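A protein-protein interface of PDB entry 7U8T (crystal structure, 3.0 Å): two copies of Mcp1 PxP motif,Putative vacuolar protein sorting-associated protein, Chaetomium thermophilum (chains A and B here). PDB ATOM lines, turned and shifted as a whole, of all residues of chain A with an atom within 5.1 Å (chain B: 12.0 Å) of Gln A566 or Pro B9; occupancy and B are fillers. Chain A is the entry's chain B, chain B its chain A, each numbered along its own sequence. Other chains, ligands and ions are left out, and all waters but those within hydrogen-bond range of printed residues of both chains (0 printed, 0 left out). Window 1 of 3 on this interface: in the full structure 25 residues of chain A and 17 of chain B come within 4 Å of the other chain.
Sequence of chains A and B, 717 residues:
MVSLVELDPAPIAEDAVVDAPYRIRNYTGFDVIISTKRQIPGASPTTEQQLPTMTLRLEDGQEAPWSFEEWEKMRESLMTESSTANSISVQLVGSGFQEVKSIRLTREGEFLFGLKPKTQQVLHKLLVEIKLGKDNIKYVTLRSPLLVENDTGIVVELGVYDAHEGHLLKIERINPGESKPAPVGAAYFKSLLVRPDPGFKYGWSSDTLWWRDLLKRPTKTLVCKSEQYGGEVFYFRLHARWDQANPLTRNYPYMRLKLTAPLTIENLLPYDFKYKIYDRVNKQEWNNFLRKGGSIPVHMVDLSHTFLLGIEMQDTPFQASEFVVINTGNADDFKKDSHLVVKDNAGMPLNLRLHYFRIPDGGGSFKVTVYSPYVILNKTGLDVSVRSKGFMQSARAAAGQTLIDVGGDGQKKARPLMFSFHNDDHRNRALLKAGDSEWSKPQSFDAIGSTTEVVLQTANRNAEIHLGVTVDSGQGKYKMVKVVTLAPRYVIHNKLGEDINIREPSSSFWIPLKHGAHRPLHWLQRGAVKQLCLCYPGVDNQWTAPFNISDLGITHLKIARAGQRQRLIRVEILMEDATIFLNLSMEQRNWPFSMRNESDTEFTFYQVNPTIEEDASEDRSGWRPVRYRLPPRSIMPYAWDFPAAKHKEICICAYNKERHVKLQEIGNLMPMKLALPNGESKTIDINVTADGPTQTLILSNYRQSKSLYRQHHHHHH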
ATOM      1  N   LYS A 558     -20.173 -31.208  16.345  1.00  0.00           N
ATOM      2  CA  LYS A 558     -21.337 -30.556  15.756  1.00  0.00           C
ATOM      3  C   LYS A 558     -21.513 -30.990  14.305  1.00  0.00           C
ATOM      4  O   LYS A 558     -20.549 -30.981  13.533  1.00  0.00           O
ATOM      5  CB  LYS A 558     -21.187 -29.037  15.823  1.00  0.00           C
ATOM      6  CG  LYS A 558     -20.717 -28.503  17.160  1.00  0.00           C
ATOM      7  CD  LYS A 558     -21.701 -27.483  17.672  1.00  0.00           C
ATOM      8  CE  LYS A 558     -21.300 -26.113  17.160  1.00  0.00           C
ATOM      9  NZ  LYS A 558     -21.770 -24.973  18.001  1.00  0.00           N
ATOM     10  N   ILE A 559     -22.743 -31.346  13.925  1.00  0.00           N
ATOM     11  CA  ILE A 559     -23.033 -31.745  12.553  1.00  0.00           C
ATOM     12  C   ILE A 559     -24.319 -31.042  12.130  1.00  0.00           C
ATOM     13  O   ILE A 559     -25.123 -30.628  12.971  1.00  0.00           O
ATOM     14  CB  ILE A 559     -23.125 -33.297  12.420  1.00  0.00           C
ATOM     15  CG1 ILE A 559     -22.955 -33.768  10.971  1.00  0.00           C
ATOM     16  CG2 ILE A 559     -24.432 -33.831  12.993  1.00  0.00           C
ATOM     17  CD1 ILE A 559     -22.691 -35.234  10.823  1.00  0.00           C
ATOM     18  N   ALA A 560     -24.479 -30.845  10.819  1.00  0.00           N
ATOM     19  CA  ALA A 560     -25.666 -30.212  10.259  1.00  0.00           C
ATOM     20  C   ALA A 560     -25.815 -30.636   8.806  1.00  0.00           C
ATOM     21  O   ALA A 560     -24.824 -30.882   8.113  1.00  0.00           O
ATOM     22  CB  ALA A 560     -25.599 -28.681  10.348  1.00  0.00           C
ATOM     23  N   GLN A 564     -29.937 -26.576   7.400  1.00  0.00           N
ATOM     24  CA  GLN A 564     -30.626 -27.059   8.583  1.00  0.00           C
ATOM     25  C   GLN A 564     -29.817 -26.696   9.822  1.00  0.00           C
ATOM     26  O   GLN A 564     -28.668 -26.253   9.735  1.00  0.00           O
ATOM     27  CB  GLN A 564     -30.870 -28.573   8.485  1.00  0.00           C
ATOM     28  CG  GLN A 564     -31.625 -28.984   7.219  1.00  0.00           C
ATOM     29  CD  GLN A 564     -32.179 -30.393   7.285  1.00  0.00           C
ATOM     30  OE1 GLN A 564     -32.405 -30.931   8.369  1.00  0.00           O
ATOM     31  NE2 GLN A 564     -32.417 -30.993   6.123  1.00  0.00           N
ATOM     32  N   ARG A 565     -30.438 -26.867  10.988  1.00  0.00           N
ATOM     33  CA  ARG A 565     -29.791 -26.504  12.239  1.00  0.00           C
ATOM     34  C   ARG A 565     -28.781 -27.573  12.645  1.00  0.00           C
ATOM     35  O   ARG A 565     -28.677 -28.640  12.034  1.00  0.00           O
ATOM     36  CB  ARG A 565     -30.826 -26.288  13.344  1.00  0.00           C
ATOM     37  CG  ARG A 565     -31.647 -27.518  13.690  1.00  0.00           C
ATOM     38  CD  ARG A 565     -32.638 -27.245  14.823  1.00  0.00           C
ATOM     39  NE  ARG A 565     -31.983 -27.017  16.106  1.00  0.00           N
ATOM     40  CZ  ARG A 565     -31.616 -27.979  16.947  1.00  0.00           C
ATOM     41  NH1 ARG A 565     -31.826 -29.257  16.670  1.00  0.00           N
ATOM     42  NH2 ARG A 565     -31.027 -27.649  18.093  1.00  0.00           N
ATOM     43  N   GLN A 566     -28.027 -27.271  13.695  1.00  0.00           N
ATOM     44  CA  GLN A 566     -26.956 -28.150  14.139  1.00  0.00           C
ATOM     45  C   GLN A 566     -27.445 -29.107  15.222  1.00  0.00           C
ATOM     46  O   GLN A 566     -28.305 -28.770  16.042  1.00  0.00           O
ATOM     47  CB  GLN A 566     -25.768 -27.337  14.659  1.00  0.00           C
ATOM     48  CG  GLN A 566     -25.102 -26.472  13.604  1.00  0.00           C
ATOM     49  CD  GLN A 566     -23.969 -25.625  14.159  1.00  0.00           C
ATOM     50  OE1 GLN A 566     -23.935 -25.314  15.347  1.00  0.00           O
ATOM     51  NE2 GLN A 566     -23.027 -25.254  13.296  1.00  0.00           N
ATOM     52  N   ARG A 567     -26.891 -30.316  15.206  1.00  0.00           N
ATOM     53  CA  ARG A 567     -27.131 -31.307  16.240  1.00  0.00           C
ATOM     54  C   ARG A 567     -25.794 -31.834  16.745  1.00  0.00           C
ATOM     55  O   ARG A 567     -24.806 -31.910  16.000  1.00  0.00           O
ATOM     56  CB  ARG A 567     -28.006 -32.465  15.735  1.00  0.00           C
ATOM     57  N   LEU A 568     -25.776 -32.194  18.022  1.00  0.00           N
ATOM     58  CA  LEU A 568     -24.554 -32.578  18.708  1.00  0.00           C
ATOM     59  C   LEU A 568     -24.416 -34.095  18.736  1.00  0.00           C
ATOM     60  O   LEU A 568     -25.379 -34.812  19.033  1.00  0.00           O
ATOM     61  CB  LEU A 568     -24.536 -31.996  20.121  1.00  0.00           C
ATOM     62  CG  LEU A 568     -23.164 -31.906  20.781  1.00  0.00           C
ATOM     63  CD1 LEU A 568     -22.204 -31.154  19.878  1.00  0.00           C
ATOM     64  CD2 LEU A 568     -23.263 -31.227  22.138  1.00  0.00           C
ATOM     65  N   TRP A 591     -26.398 -29.024  25.986  1.00  0.00           N
ATOM     66  CA  TRP A 591     -25.119 -28.754  25.352  1.00  0.00           C
ATOM     67  C   TRP A 591     -24.138 -28.184  26.382  1.00  0.00           C
ATOM     68  O   TRP A 591     -24.570 -27.631  27.398  1.00  0.00           O
ATOM     69  CB  TRP A 591     -25.339 -27.780  24.188  1.00  0.00           C
ATOM     70  CG  TRP A 591     -25.872 -28.431  22.936  1.00  0.00           C
ATOM     71  CD1 TRP A 591     -26.689 -29.520  22.856  1.00  0.00           C
ATOM     72  CD2 TRP A 591     -25.603 -28.037  21.583  1.00  0.00           C
ATOM     73  NE1 TRP A 591     -26.953 -29.821  21.543  1.00  0.00           N
ATOM     74  CE2 TRP A 591     -26.298 -28.927  20.741  1.00  0.00           C
ATOM     75  CE3 TRP A 591     -24.841 -27.019  21.005  1.00  0.00           C
ATOM     76  CZ2 TRP A 591     -26.254 -28.827  19.353  1.00  0.00           C
ATOM     77  CZ3 TRP A 591     -24.797 -26.923  19.631  1.00  0.00           C
ATOM     78  CH2 TRP A 591     -25.496 -27.823  18.819  1.00  0.00           C
ATOM     79  N   TYR A 628     -21.226 -16.671  14.931  1.00  0.00           N
ATOM     80  CA  TYR A 628     -22.605 -16.811  15.367  1.00  0.00           C
ATOM     81  C   TYR A 628     -23.124 -15.452  15.811  1.00  0.00           C
ATOM     82  O   TYR A 628     -22.385 -14.662  16.409  1.00  0.00           O
ATOM     83  CB  TYR A 628     -22.727 -17.827  16.518  1.00  0.00           C
ATOM     84  CG  TYR A 628     -22.298 -19.236  16.167  1.00  0.00           C
ATOM     85  CD1 TYR A 628     -20.958 -19.623  16.224  1.00  0.00           C
ATOM     86  CD2 TYR A 628     -23.239 -20.186  15.790  1.00  0.00           C
ATOM     87  CE1 TYR A 628     -20.570 -20.913  15.895  1.00  0.00           C
ATOM     88  CE2 TYR A 628     -22.862 -21.479  15.457  1.00  0.00           C
ATOM     89  CZ  TYR A 628     -21.527 -21.837  15.514  1.00  0.00           C
ATOM     90  OH  TYR A 628     -21.157 -23.125  15.188  1.00  0.00           O
ATOM     91  N   MET A 636     -28.604 -19.141  23.424  1.00  0.00           N
ATOM     92  CA  MET A 636     -28.352 -20.194  22.404  1.00  0.00           C
ATOM     93  C   MET A 636     -27.281 -21.158  22.925  1.00  0.00           C
ATOM     94  O   MET A 636     -26.216 -20.682  23.367  1.00  0.00           O
ATOM     95  CB  MET A 636     -27.880 -19.578  21.085  1.00  0.00           C
ATOM     96  CG  MET A 636     -27.525 -20.610  20.034  1.00  0.00           C
ATOM     97  SD  MET A 636     -25.745 -20.676  19.707  1.00  0.00           S
ATOM     98  CE  MET A 636     -25.646 -19.639  18.248  1.00  0.00           C
ATOM     99  N   PRO A 637     -27.516 -22.489  22.886  1.00  0.00           N
ATOM    100  CA  PRO A 637     -26.521 -23.466  23.330  1.00  0.00           C
ATOM    101  C   PRO A 637     -25.397 -23.590  22.294  1.00  0.00           C
ATOM    102  O   PRO A 637     -25.685 -23.548  21.112  1.00  0.00           O
ATOM    103  CB  PRO A 637     -27.318 -24.774  23.388  1.00  0.00           C
ATOM    104  CG  PRO A 637     -28.383 -24.593  22.329  1.00  0.00           C
ATOM    105  CD  PRO A 637     -28.742 -23.122  22.395  1.00  0.00           C
ATOM    106  N   VAL B   5     -35.102 -14.818  24.430  1.00  0.00           N
ATOM    107  CA  VAL B   5     -35.552 -15.468  23.203  1.00  0.00           C
ATOM    108  C   VAL B   5     -34.629 -16.640  22.900  1.00  0.00           C
ATOM    109  O   VAL B   5     -33.433 -16.456  22.653  1.00  0.00           O
ATOM    110  CB  VAL B   5     -35.586 -14.476  22.032  1.00  0.00           C
ATOM    111  CG1 VAL B   5     -35.985 -15.182  20.745  1.00  0.00           C
ATOM    112  CG2 VAL B   5     -36.545 -13.333  22.338  1.00  0.00           C
ATOM    113  N   GLU B   6     -35.185 -17.847  22.912  1.00  0.00           N
ATOM    114  CA  GLU B   6     -34.402 -19.053  22.683  1.00  0.00           C
ATOM    115  C   GLU B   6     -34.168 -19.245  21.190  1.00  0.00           C
ATOM    116  O   GLU B   6     -35.117 -19.235  20.399  1.00  0.00           O
ATOM    117  CB  GLU B   6     -35.121 -20.263  23.276  1.00  0.00           C
ATOM    118  CG  GLU B   6     -35.245 -20.208  24.787  1.00  0.00           C
ATOM    119  CD  GLU B   6     -36.014 -21.381  25.346  1.00  0.00           C
ATOM    120  OE1 GLU B   6     -36.598 -22.141  24.544  1.00  0.00           O
ATOM    121  OE2 GLU B   6     -36.044 -21.539  26.586  1.00  0.00           O
ATOM    122  N   LEU B   7     -32.905 -19.412  20.807  1.00  0.00           N
ATOM    123  CA  LEU B   7     -32.527 -19.564  19.410  1.00  0.00           C
ATOM    124  C   LEU B   7     -31.918 -20.933  19.159  1.00  0.00           C
ATOM    125  O   LEU B   7     -31.329 -21.549  20.052  1.00  0.00           O
ATOM    126  CB  LEU B   7     -31.529 -18.497  18.981  1.00  0.00           C
ATOM    127  CG  LEU B   7     -31.802 -17.087  19.481  1.00  0.00           C
ATOM    128  CD1 LEU B   7     -30.613 -16.242  19.160  1.00  0.00           C
ATOM    129  CD2 LEU B   7     -33.040 -16.534  18.810  1.00  0.00           C
ATOM    130  N   ASP B   8     -32.071 -21.398  17.925  1.00  0.00           N
ATOM    131  CA  ASP B   8     -31.398 -22.608  17.497  1.00  0.00           C
ATOM    132  C   ASP B   8     -29.912 -22.312  17.287  1.00  0.00           C
ATOM    133  O   ASP B   8     -29.541 -21.187  16.936  1.00  0.00           O
ATOM    134  CB  ASP B   8     -32.035 -23.139  16.213  1.00  0.00           C
ATOM    135  CG  ASP B   8     -33.267 -23.993  16.485  1.00  0.00           C
ATOM    136  OD1 ASP B   8     -33.277 -24.731  17.496  1.00  0.00           O
ATOM    137  OD2 ASP B   8     -34.225 -23.928  15.684  1.00  0.00           O
ATOM    138  N   PRO B   9     -29.027 -23.304  17.498  1.00  0.00           N
ATOM    139  CA  PRO B   9     -27.585 -23.021  17.411  1.00  0.00           C
ATOM    140  C   PRO B   9     -26.998 -22.969  16.005  1.00  0.00           C
ATOM    141  O   PRO B   9     -25.806 -23.234  15.847  1.00  0.00           O
ATOM    142  CB  PRO B   9     -26.967 -24.173  18.211  1.00  0.00           C
ATOM    143  CG  PRO B   9     -27.926 -25.279  18.043  1.00  0.00           C
ATOM    144  CD  PRO B   9     -29.275 -24.638  18.078  1.00  0.00           C
ATOM    145  N   ALA B  10     -27.784 -22.615  14.990  1.00  0.00           N
ATOM    146  CA  ALA B  10     -27.289 -22.532  13.623  1.00  0.00           C
ATOM    147  C   ALA B  10     -26.420 -21.285  13.430  1.00  0.00           C
ATOM    148  O   ALA B  10     -26.680 -20.241  14.034  1.00  0.00           O
ATOM    149  CB  ALA B  10     -28.460 -22.509  12.646  1.00  0.00           C
ATOM    150  N   PRO B  11     -25.365 -21.368  12.591  1.00  0.00           N
ATOM    151  CA  PRO B  11     -24.479 -20.205  12.407  1.00  0.00           C
ATOM    152  C   PRO B  11     -25.032 -19.103  11.512  1.00  0.00           C
ATOM    153  O   PRO B  11     -26.216 -19.097  11.158  1.00  0.00           O
ATOM    154  CB  PRO B  11     -23.218 -20.826  11.794  1.00  0.00           C
ATOM    155  CG  PRO B  11     -23.699 -22.033  11.094  1.00  0.00           C
ATOM    156  CD  PRO B  11     -24.826 -22.572  11.931  1.00  0.00           C
ATOM    157  N   ILE B  12     -24.171 -18.155  11.148  1.00  0.00           N
ATOM    158  CA  ILE B  12     -24.579 -17.003  10.341  1.00  0.00           C
ATOM    159  C   ILE B  12     -24.610 -17.379   8.861  1.00  0.00           C
ATOM    160  O   ILE B  12     -23.671 -17.985   8.345  1.00  0.00           O
ATOM    161  CB  ILE B  12     -23.647 -15.784  10.592  1.00  0.00           C
ATOM    162  CG1 ILE B  12     -24.023 -15.085  11.903  1.00  0.00           C
ATOM    163  CG2 ILE B  12     -23.716 -14.793   9.441  1.00  0.00           C
ATOM    164  CD1 ILE B  12     -23.145 -13.906  12.256  1.00  0.00           C
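The side-chain carboxylate of Asp B8 lies within salt-bridge range of the guanidinium group of Arg A565, 3.0 Å away. The side-chain amide oxygen (OE1) of Gln A566 lies close to the backbone carbonyl oxygen (O) of Pro B9 (2.8 Å).
Among the printed residues, merely in contact across the chains: Arg A565 with Pro B9 (3.5 Å), Gln A566 with Pro B11 (3.5 Å), Trp A591 with Pro B9 (3.6 Å), Tyr A628 with Pro B9 (3.4 Å), Tyr A628 with Ala B10 (3.9 Å), Tyr A628 with Pro B11 (3.6 Å), Tyr A628 with Ile B12 (3.9 Å), Met A636 with Leu B7 (3.9 Å), Met A636 with Asp B8 (3.7 Å), Met A636 with Pro B9 (3.6 Å), Pro A637 with Leu B7 (3.8 Å) and Pro A637 with Pro B9 (3.2 Å).
No position is printed for both chains. Of the 14 pairs that touch across the chains among the printed residues, none has its exchanged pair printed and touching as well.
NZ of Lys A558 sits close to OE1 of Gln A566, at 3.4 Å. The side-chain hydroxyl (OH) of Tyr A628 lies within hydrogen-bond range of the side-chain amino group (NZ) of Lys A558 (3.4 Å). The side-chain amide nitrogen of Gln A566 sits at hydrogen-bond distance from the side-chain hydroxyl of Tyr A628, at 3.4 Å.
Of the 8 printed residues of chain B, 6 touch a printed residue of chain A. Hydrophobic or aromatic side chains of chain B that line the printed part of chain A: Pro B9, Pro B11 and Ile B12. Hydrophobic or aromatic side chains of chain A within 4 Å of the printed part of chain B: Trp A591, Tyr A628, Met A636 and Pro A637.
No residue of chain B comes within 4 Å of Lys A558. Of chain B, only Asp B8 and Pro B9 come within 4 Å of Arg A565. Printed residues of chain B within 4 Å of Gln A566: Pro B9 (2.8 Å) and Pro B11 (3.5 Å). Arg A567 touches none of the printed residues of chain B. Of the printed residues of chain B, Trp A591 touches Pro B9 (3.6 Å). Of the printed residues of chain B, Tyr A628 touches Pro B9, Ala B10, Pro B11 and Ile B12. Met A636 touches just these residues of chain B: Leu B7, Asp B8 and Pro B9. Of the printed residues of chain A, Leu B7 touches Met A636 (3.9 Å) and Pro A637 (3.8 Å). Pro B9 touches six residues of chain A. Printed residues of chain A within 4 Å of Ala B10: Tyr A628 (3.9 Å). Of the printed residues of chain A, Ile B12 touches Tyr A628. The nearest printed residue of chain A that does not touch Ile B12 is Met A636 (7.4 Å).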
